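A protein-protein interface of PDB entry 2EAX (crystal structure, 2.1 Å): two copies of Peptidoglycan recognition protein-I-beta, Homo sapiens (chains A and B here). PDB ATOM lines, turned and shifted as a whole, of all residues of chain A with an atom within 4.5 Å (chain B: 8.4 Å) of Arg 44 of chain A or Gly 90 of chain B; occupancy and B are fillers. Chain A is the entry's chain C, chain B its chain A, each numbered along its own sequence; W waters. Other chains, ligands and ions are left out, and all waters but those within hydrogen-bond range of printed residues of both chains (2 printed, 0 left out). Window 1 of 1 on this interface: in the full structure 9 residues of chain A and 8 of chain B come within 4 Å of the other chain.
OD2 of Asp 93 of chain B lies within salt-bridge range of NH1 of Arg 44 of chain A.
N of Lys 25 of chain B sits at hydrogen-bond distance from O of Ile 94 of chain B (3.3 Å).
O of Ile 94 of chain B sits at hydrogen-bond distance from N of Tyr 26 of chain B, 3.2 Å away.
The backbone carbonyl oxygen (O) of Arg 44 of chain A is in hydrogen-bond range of the guanidinium group (NH1) of Arg 48 of chain A.
CG2 of Val 9 of chain A touches OH of Tyr 26 of chain B, 3.7 Å away.
Ser 40 of chain A touches Gly 90 of chain B (OG to CA, 3.5 Å).
OD1 of Asp 93 of chain B touches CB of Ser 40 of chain A, 3.4 Å away.
CB of Asp 41 of chain A touches OD2 of Asp 93 of chain B, 3.4 Å away.
O of Gly 90 of chain B touches NH2 of Arg 44 of chain A, 3.6 Å away.
Ile 94 of chain B touches Arg 44 of chain A.
Ala 74 of chain A touches Pro 89 of chain B.
Printed residues of chain B within 4 Å of Ser 40 of chain A: Gly 90 (3.5 Å) and Asp 93 (3.4 Å).
Of chain B, only Gly 90 (3.6 Å), Asp 93 (3.0 Å) and Ile 94 (3.7 Å) come within 4 Å of Arg 44 of chain A.
Leu 46 of chain A touches none of the printed residues of chain B.
Lys 25 of chain B touches none of the printed residues of chain A.
Of the printed residues of chain A, Asp 93 of chain B touches Ser 40 (3.4 Å), Asp 41 (3.4 Å) and Arg 44 (3.0 Å).
The nearest residue of chain A that does not touch Gly 90 of chain B is Ala 74 of chain A (4.4 Å).
Of the 13 printed residues of chain B, 5 touch a printed residue of chain A.
Hydrophobic or aromatic side chains of chain B that line the printed part of chain A: Tyr 26 and Ile 94.
Of the 13 printed residues of chain A, 5 touch a printed residue of chain B.
Along chain A the printed residues that touch a printed residue of chain B span positions 9 to 74.
Among the printed residues, 8 pairs touch across the chains.
Among the printed residues, Asp or Glu carboxylates within 4 Å of a Lys or Arg side-chain nitrogen of the other chain: Arg 44 of chain A with Asp 93 of chain B (3.0 Å).
No position is printed for both chains.
Water W2 lies within hydrogen-bond range of OG of Ser 40 of chain A (2.5 Å), N of Asp 92 of chain B (3.2 Å) and N of Gly 90 of chain B (3.4 Å).
Water W1 lies within hydrogen-bond range of the guanidinium group of Arg 44 of chain A (2.7 Å), the backbone carbonyl oxygen of Gly 90 of chain B (2.9 Å) and the side-chain hydroxyl of Tyr 76 of chain A (3.1 Å).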
ATOM      1  N   VAL A   9       5.572 -13.970 -19.730  1.00  0.00           N
ATOM      2  CA  VAL A   9       4.589 -13.208 -18.963  1.00  0.00           C
ATOM      3  C   VAL A   9       3.138 -13.708 -19.078  1.00  0.00           C
ATOM      4  O   VAL A   9       2.413 -13.721 -18.069  1.00  0.00           O
ATOM      5  CB  VAL A   9       4.621 -11.708 -19.331  1.00  0.00           C
ATOM      6  CG1 VAL A   9       3.598 -10.956 -18.506  1.00  0.00           C
ATOM      7  CG2 VAL A   9       6.001 -11.133 -19.063  1.00  0.00           C
ATOM      8  N   TRP A  10       2.705 -14.075 -20.288  1.00  0.00           N
ATOM      9  CA  TRP A  10       1.354 -14.611 -20.491  1.00  0.00           C
ATOM     10  C   TRP A  10       1.341 -16.144 -20.437  1.00  0.00           C
ATOM     11  O   TRP A  10       0.308 -16.770 -20.699  1.00  0.00           O
ATOM     12  CB  TRP A  10       0.722 -14.158 -21.837  1.00  0.00           C
ATOM     13  CG  TRP A  10       1.470 -14.510 -23.104  1.00  0.00           C
ATOM     14  CD1 TRP A  10       2.456 -13.777 -23.699  1.00  0.00           C
ATOM     15  CD2 TRP A  10       1.254 -15.656 -23.964  1.00  0.00           C
ATOM     16  NE1 TRP A  10       2.862 -14.383 -24.871  1.00  0.00           N
ATOM     17  CE2 TRP A  10       2.144 -15.535 -25.053  1.00  0.00           C
ATOM     18  CE3 TRP A  10       0.398 -16.764 -23.915  1.00  0.00           C
ATOM     19  CZ2 TRP A  10       2.204 -16.483 -26.088  1.00  0.00           C
ATOM     20  CZ3 TRP A  10       0.455 -17.709 -24.946  1.00  0.00           C
ATOM     21  CH2 TRP A  10       1.353 -17.560 -26.016  1.00  0.00           C
ATOM     22  N   SER A  40      -6.055  -6.140 -19.508  1.00  0.00           N
ATOM     23  CA  SER A  40      -4.820  -6.931 -19.451  1.00  0.00           C
ATOM     24  C   SER A  40      -4.938  -8.411 -19.086  1.00  0.00           C
ATOM     25  O   SER A  40      -4.752  -9.283 -19.941  1.00  0.00           O
ATOM     26  CB  SER A  40      -3.821  -6.263 -18.497  1.00  0.00           C
ATOM     27  OG  SER A  40      -3.393  -5.011 -19.006  1.00  0.00           O
ATOM     28  N   ASP A  41      -5.225  -8.694 -17.818  1.00  0.00           N
ATOM     29  CA  ASP A  41      -5.342 -10.076 -17.359  1.00  0.00           C
ATOM     30  C   ASP A  41      -6.256 -10.899 -18.263  1.00  0.00           C
ATOM     31  O   ASP A  41      -6.112 -12.118 -18.362  1.00  0.00           O
ATOM     32  CB  ASP A  41      -5.855 -10.110 -15.914  1.00  0.00           C
ATOM     33  CG  ASP A  41      -7.319  -9.736 -15.801  1.00  0.00           C
ATOM     34  OD1 ASP A  41      -7.749  -8.793 -16.502  1.00  0.00           O
ATOM     35  OD2 ASP A  41      -8.036 -10.381 -15.000  1.00  0.00           O
ATOM     36  N   GLU A  42      -7.191 -10.225 -18.929  1.00  0.00           N
ATOM     37  CA  GLU A  42      -8.127 -10.890 -19.830  1.00  0.00           C
ATOM     38  C   GLU A  42      -7.483 -11.217 -21.170  1.00  0.00           C
ATOM     39  O   GLU A  42      -7.796 -12.236 -21.777  1.00  0.00           O
ATOM     40  CB  GLU A  42      -9.366 -10.016 -20.048  1.00  0.00           C
ATOM     41  CG  GLU A  42     -10.232 -10.430 -21.231  1.00  0.00           C
ATOM     42  CD  GLU A  42     -11.438  -9.529 -21.417  1.00  0.00           C
ATOM     43  OE1 GLU A  42     -11.275  -8.294 -21.385  1.00  0.00           O
ATOM     44  OE2 GLU A  42     -12.553 -10.057 -21.603  1.00  0.00           O
ATOM     45  N   CYS A  43      -6.592 -10.349 -21.638  1.00  0.00           N
ATOM     46  CA  CYS A  43      -5.911 -10.591 -22.909  1.00  0.00           C
ATOM     47  C   CYS A  43      -4.879 -11.712 -22.783  1.00  0.00           C
ATOM     48  O   CYS A  43      -4.768 -12.552 -23.675  1.00  0.00           O
ATOM     49  CB  CYS A  43      -5.219  -9.324 -23.413  1.00  0.00           C
ATOM     50  SG  CYS A  43      -6.287  -8.014 -24.101  1.00  0.00           S
ATOM     51  N   ARG A  44      -4.128 -11.719 -21.680  1.00  0.00           N
ATOM     52  CA  ARG A  44      -3.113 -12.748 -21.457  1.00  0.00           C
ATOM     53  C   ARG A  44      -3.727 -14.127 -21.675  1.00  0.00           C
ATOM     54  O   ARG A  44      -3.092 -15.018 -22.236  1.00  0.00           O
ATOM     55  CB  ARG A  44      -2.523 -12.658 -20.034  1.00  0.00           C
ATOM     56  CG  ARG A  44      -1.621 -11.435 -19.782  1.00  0.00           C
ATOM     57  CD  ARG A  44      -0.695 -11.618 -18.557  1.00  0.00           C
ATOM     58  NE  ARG A  44      -1.365 -11.464 -17.262  1.00  0.00           N
ATOM     59  CZ  ARG A  44      -1.657 -10.296 -16.701  1.00  0.00           C
ATOM     60  NH1 ARG A  44      -2.269 -10.253 -15.525  1.00  0.00           N
ATOM     61  NH2 ARG A  44      -1.326  -9.165 -17.306  1.00  0.00           N
ATOM     62  N   LEU A  45      -4.979 -14.278 -21.253  1.00  0.00           N
ATOM     63  CA  LEU A  45      -5.716 -15.537 -21.386  1.00  0.00           C
ATOM     64  C   LEU A  45      -6.173 -15.849 -22.823  1.00  0.00           C
ATOM     65  O   LEU A  45      -6.229 -17.012 -23.220  1.00  0.00           O
ATOM     66  CB  LEU A  45      -6.932 -15.514 -20.450  1.00  0.00           C
ATOM     67  CG  LEU A  45      -7.878 -16.713 -20.493  1.00  0.00           C
ATOM     68  CD1 LEU A  45      -7.179 -17.975 -19.981  1.00  0.00           C
ATOM     69  CD2 LEU A  45      -9.093 -16.398 -19.660  1.00  0.00           C
ATOM     70  N   LEU A  46      -6.502 -14.818 -23.596  1.00  0.00           N
ATOM     71  CA  LEU A  46      -6.951 -15.015 -24.974  1.00  0.00           C
ATOM     72  C   LEU A  46      -5.807 -15.509 -25.860  1.00  0.00           C
ATOM     73  O   LEU A  46      -6.037 -16.201 -26.844  1.00  0.00           O
ATOM     74  CB  LEU A  46      -7.503 -13.702 -25.551  1.00  0.00           C
ATOM     75  CG  LEU A  46      -8.683 -13.745 -26.534  1.00  0.00           C
ATOM     76  CD1 LEU A  46      -8.872 -12.370 -27.164  1.00  0.00           C
ATOM     77  CD2 LEU A  46      -8.442 -14.777 -27.617  1.00  0.00           C
ATOM     78  N   VAL A  47      -4.573 -15.144 -25.513  1.00  0.00           N
ATOM     79  CA  VAL A  47      -3.411 -15.554 -26.297  1.00  0.00           C
ATOM     80  C   VAL A  47      -3.065 -17.016 -26.007  1.00  0.00           C
ATOM     81  O   VAL A  47      -2.595 -17.748 -26.888  1.00  0.00           O
ATOM     82  CB  VAL A  47      -2.170 -14.664 -25.991  1.00  0.00           C
ATOM     83  CG1 VAL A  47      -1.023 -15.039 -26.923  1.00  0.00           C
ATOM     84  CG2 VAL A  47      -2.517 -13.187 -26.174  1.00  0.00           C
ATOM     85  N   ARG A  48      -3.297 -17.439 -24.772  1.00  0.00           N
ATOM     86  CA  ARG A  48      -3.028 -18.822 -24.399  1.00  0.00           C
ATOM     87  C   ARG A  48      -3.980 -19.728 -25.190  1.00  0.00           C
ATOM     88  O   ARG A  48      -3.564 -20.756 -25.723  1.00  0.00           O
ATOM     89  CB  ARG A  48      -3.202 -19.023 -22.876  1.00  0.00           C
ATOM     90  CG  ARG A  48      -2.168 -18.272 -22.017  1.00  0.00           C
ATOM     91  CD  ARG A  48      -2.105 -18.784 -20.563  1.00  0.00           C
ATOM     92  NE  ARG A  48      -3.135 -18.240 -19.680  1.00  0.00           N
ATOM     93  CZ  ARG A  48      -3.081 -17.032 -19.117  1.00  0.00           C
ATOM     94  NH1 ARG A  48      -2.045 -16.235 -19.343  1.00  0.00           N
ATOM     95  NH2 ARG A  48      -4.061 -16.614 -18.321  1.00  0.00           N
ATOM     96  N   ALA A  74      -2.045  -2.953 -25.855  1.00  0.00           N
ATOM     97  CA  ALA A  74      -0.748  -3.623 -25.731  1.00  0.00           C
ATOM     98  C   ALA A  74      -0.552  -4.688 -26.797  1.00  0.00           C
ATOM     99  O   ALA A  74      -1.523  -5.247 -27.315  1.00  0.00           O
ATOM    100  CB  ALA A  74      -0.601  -4.239 -24.345  1.00  0.00           C
ATOM    101  N   TYR A  76       1.162  -8.384 -28.046  1.00  0.00           N
ATOM    102  CA  TYR A  76       1.529  -9.690 -27.494  1.00  0.00           C
ATOM    103  C   TYR A  76       2.314 -10.561 -28.480  1.00  0.00           C
ATOM    104  O   TYR A  76       1.913 -10.728 -29.635  1.00  0.00           O
ATOM    105  CB  TYR A  76       0.272 -10.443 -27.021  1.00  0.00           C
ATOM    106  CG  TYR A  76      -0.408  -9.803 -25.826  1.00  0.00           C
ATOM    107  CD1 TYR A  76      -1.132  -8.617 -25.960  1.00  0.00           C
ATOM    108  CD2 TYR A  76      -0.306 -10.373 -24.555  1.00  0.00           C
ATOM    109  CE1 TYR A  76      -1.731  -8.012 -24.866  1.00  0.00           C
ATOM    110  CE2 TYR A  76      -0.903  -9.774 -23.446  1.00  0.00           C
ATOM    111  CZ  TYR A  76      -1.612  -8.592 -23.611  1.00  0.00           C
ATOM    112  OH  TYR A  76      -2.196  -7.990 -22.522  1.00  0.00           O
ATOM    113  N   LYS B  25       4.035  -8.749  -8.767  1.00  0.00           N
ATOM    114  CA  LYS B  25       5.253  -9.376  -9.277  1.00  0.00           C
ATOM    115  C   LYS B  25       6.327  -8.420  -9.798  1.00  0.00           C
ATOM    116  O   LYS B  25       7.503  -8.779  -9.835  1.00  0.00           O
ATOM    117  CB  LYS B  25       4.909 -10.395 -10.368  1.00  0.00           C
ATOM    118  CG  LYS B  25       4.082  -9.850 -11.520  1.00  0.00           C
ATOM    119  CD  LYS B  25       3.932 -10.890 -12.626  1.00  0.00           C
ATOM    120  CE  LYS B  25       3.213 -12.136 -12.142  1.00  0.00           C
ATOM    121  NZ  LYS B  25       1.848 -11.828 -11.628  1.00  0.00           N
ATOM    122  N   TYR B  26       5.933  -7.215 -10.202  1.00  0.00           N
ATOM    123  CA  TYR B  26       6.899  -6.248 -10.713  1.00  0.00           C
ATOM    124  C   TYR B  26       6.982  -4.954  -9.894  1.00  0.00           C
ATOM    125  O   TYR B  26       6.046  -4.578  -9.189  1.00  0.00           O
ATOM    126  CB  TYR B  26       6.597  -5.892 -12.179  1.00  0.00           C
ATOM    127  CG  TYR B  26       6.871  -7.000 -13.189  1.00  0.00           C
ATOM    128  CD1 TYR B  26       5.999  -8.079 -13.333  1.00  0.00           C
ATOM    129  CD2 TYR B  26       8.006  -6.964 -13.998  1.00  0.00           C
ATOM    130  CE1 TYR B  26       6.252  -9.098 -14.261  1.00  0.00           C
ATOM    131  CE2 TYR B  26       8.267  -7.974 -14.925  1.00  0.00           C
ATOM    132  CZ  TYR B  26       7.387  -9.038 -15.053  1.00  0.00           C
ATOM    133  OH  TYR B  26       7.651 -10.036 -15.969  1.00  0.00           O
ATOM    134  N   ILE B  28       8.230  -0.979 -10.603  1.00  0.00           N
ATOM    135  CA  ILE B  28       8.627  -0.071 -11.675  1.00  0.00           C
ATOM    136  C   ILE B  28       9.121   1.304 -11.238  1.00  0.00           C
ATOM    137  O   ILE B  28       8.387   2.088 -10.632  1.00  0.00           O
ATOM    138  CB  ILE B  28       7.462   0.092 -12.672  1.00  0.00           C
ATOM    139  CG1 ILE B  28       6.975  -1.300 -13.095  1.00  0.00           C
ATOM    140  CG2 ILE B  28       7.905   0.891 -13.900  1.00  0.00           C
ATOM    141  CD1 ILE B  28       5.768  -1.291 -14.011  1.00  0.00           C
ATOM    142  N   SER B  87       0.426   3.521 -16.062  1.00  0.00           N
ATOM    143  CA  SER B  87       1.639   4.055 -16.676  1.00  0.00           C
ATOM    144  C   SER B  87       2.376   3.066 -17.568  1.00  0.00           C
ATOM    145  O   SER B  87       3.272   3.461 -18.311  1.00  0.00           O
ATOM    146  CB  SER B  87       2.607   4.557 -15.596  1.00  0.00           C
ATOM    147  OG  SER B  87       3.251   3.482 -14.924  1.00  0.00           O
ATOM    148  N   THR B  88       2.006   1.788 -17.488  1.00  0.00           N
ATOM    149  CA  THR B  88       2.634   0.736 -18.290  1.00  0.00           C
ATOM    150  C   THR B  88       1.574  -0.232 -18.836  1.00  0.00           C
ATOM    151  O   THR B  88       1.200  -1.190 -18.161  1.00  0.00           O
ATOM    152  CB  THR B  88       3.633  -0.086 -17.441  1.00  0.00           C
ATOM    153  OG1 THR B  88       4.511   0.798 -16.727  1.00  0.00           O
ATOM    154  CG2 THR B  88       4.460  -1.005 -18.335  1.00  0.00           C
ATOM    155  N   PRO B  89       1.088  -0.003 -20.073  1.00  0.00           N
ATOM    156  CA  PRO B  89       0.069  -0.863 -20.687  1.00  0.00           C
ATOM    157  C   PRO B  89       0.429  -2.351 -20.754  1.00  0.00           C
ATOM    158  O   PRO B  89       1.338  -2.754 -21.484  1.00  0.00           O
ATOM    159  CB  PRO B  89      -0.104  -0.254 -22.077  1.00  0.00           C
ATOM    160  CG  PRO B  89       0.212   1.193 -21.851  1.00  0.00           C
ATOM    161  CD  PRO B  89       1.431   1.111 -20.975  1.00  0.00           C
ATOM    162  N   GLY B  90      -0.302  -3.162 -19.996  1.00  0.00           N
ATOM    163  CA  GLY B  90      -0.059  -4.593 -19.988  1.00  0.00           C
ATOM    164  C   GLY B  90       0.592  -5.121 -18.725  1.00  0.00           C
ATOM    165  O   GLY B  90       0.625  -6.335 -18.516  1.00  0.00           O
ATOM    166  N   TYR B  91       1.109  -4.217 -17.891  1.00  0.00           N
ATOM    167  CA  TYR B  91       1.769  -4.590 -16.637  1.00  0.00           C
ATOM    168  C   TYR B  91       1.128  -3.913 -15.416  1.00  0.00           C
ATOM    169  O   TYR B  91       1.509  -4.185 -14.278  1.00  0.00           O
ATOM    170  CB  TYR B  91       3.261  -4.207 -16.676  1.00  0.00           C
ATOM    171  CG  TYR B  91       4.120  -4.976 -17.665  1.00  0.00           C
ATOM    172  CD1 TYR B  91       4.080  -4.695 -19.031  1.00  0.00           C
ATOM    173  CD2 TYR B  91       4.991  -5.979 -17.227  1.00  0.00           C
ATOM    174  CE1 TYR B  91       4.888  -5.386 -19.937  1.00  0.00           C
ATOM    175  CE2 TYR B  91       5.799  -6.674 -18.119  1.00  0.00           C
ATOM    176  CZ  TYR B  91       5.744  -6.374 -19.472  1.00  0.00           C
ATOM    177  OH  TYR B  91       6.553  -7.063 -20.356  1.00  0.00           O
ATOM    178  N   ASP B  92       0.155  -3.038 -15.667  1.00  0.00           N
ATOM    179  CA  ASP B  92      -0.544  -2.283 -14.622  1.00  0.00           C
ATOM    180  C   ASP B  92      -1.211  -3.086 -13.498  1.00  0.00           C
ATOM    181  O   ASP B  92      -1.082  -2.740 -12.320  1.00  0.00           O
ATOM    182  CB  ASP B  92      -1.589  -1.366 -15.269  1.00  0.00           C
ATOM    183  CG  ASP B  92      -0.971  -0.141 -15.931  1.00  0.00           C
ATOM    184  OD1 ASP B  92      -1.472   0.288 -16.996  1.00  0.00           O
ATOM    185  OD2 ASP B  92       0.007   0.402 -15.378  1.00  0.00           O
ATOM    186  N   ASP B  93      -1.922  -4.154 -13.847  1.00  0.00           N
ATOM    187  CA  ASP B  93      -2.599  -4.945 -12.828  1.00  0.00           C
ATOM    188  C   ASP B  93      -1.691  -5.895 -12.052  1.00  0.00           C
ATOM    189  O   ASP B  93      -2.167  -6.653 -11.206  1.00  0.00           O
ATOM    190  CB  ASP B  93      -3.758  -5.720 -13.453  1.00  0.00           C
ATOM    191  CG  ASP B  93      -3.295  -6.748 -14.457  1.00  0.00           C
ATOM    192  OD1 ASP B  93      -2.517  -6.389 -15.363  1.00  0.00           O
ATOM    193  OD2 ASP B  93      -3.715  -7.913 -14.339  1.00  0.00           O
ATOM    194  N   ILE B  94      -0.389  -5.836 -12.319  1.00  0.00           N
ATOM    195  CA  ILE B  94       0.572  -6.706 -11.643  1.00  0.00           C
ATOM    196  C   ILE B  94       1.880  -6.001 -11.249  1.00  0.00           C
ATOM    197  O   ILE B  94       2.915  -6.653 -11.108  1.00  0.00           O
ATOM    198  CB  ILE B  94       0.940  -7.916 -12.538  1.00  0.00           C
ATOM    199  CG1 ILE B  94       1.582  -7.413 -13.837  1.00  0.00           C
ATOM    200  CG2 ILE B  94      -0.299  -8.743 -12.827  1.00  0.00           C
ATOM    201  CD1 ILE B  94       2.128  -8.503 -14.728  1.00  0.00           C
ATOM    202  N   ALA B  95       1.834  -4.683 -11.062  1.00  0.00           N
ATOM    203  CA  ALA B  95       3.032  -3.930 -10.709  1.00  0.00           C
ATOM    204  C   ALA B  95       2.770  -2.720  -9.819  1.00  0.00           C
ATOM    205  O   ALA B  95       1.647  -2.233  -9.726  1.00  0.00           O
ATOM    206  CB  ALA B  95       3.745  -3.489 -11.968  1.00  0.00           C
ATOM    207  N   VAL B 142       9.809  -1.975 -20.134  1.00  0.00           N
ATOM    208  CA  VAL B 142       8.480  -2.460 -20.487  1.00  0.00           C
ATOM    209  C   VAL B 142       7.519  -1.417 -21.059  1.00  0.00           C
ATOM    210  O   VAL B 142       6.300  -1.563 -20.941  1.00  0.00           O
ATOM    211  CB  VAL B 142       7.816  -3.103 -19.254  1.00  0.00           C
ATOM    212  CG1 VAL B 142       8.593  -4.342 -18.837  1.00  0.00           C
ATOM    213  CG2 VAL B 142       7.774  -2.094 -18.099  1.00  0.00           C
HETATM  214  O   HOH W   1      -0.804  -8.438 -19.814  1.00  0.00           O
HETATM  215  O   HOH W   2      -2.549  -3.352 -17.398  1.00  0.00           O
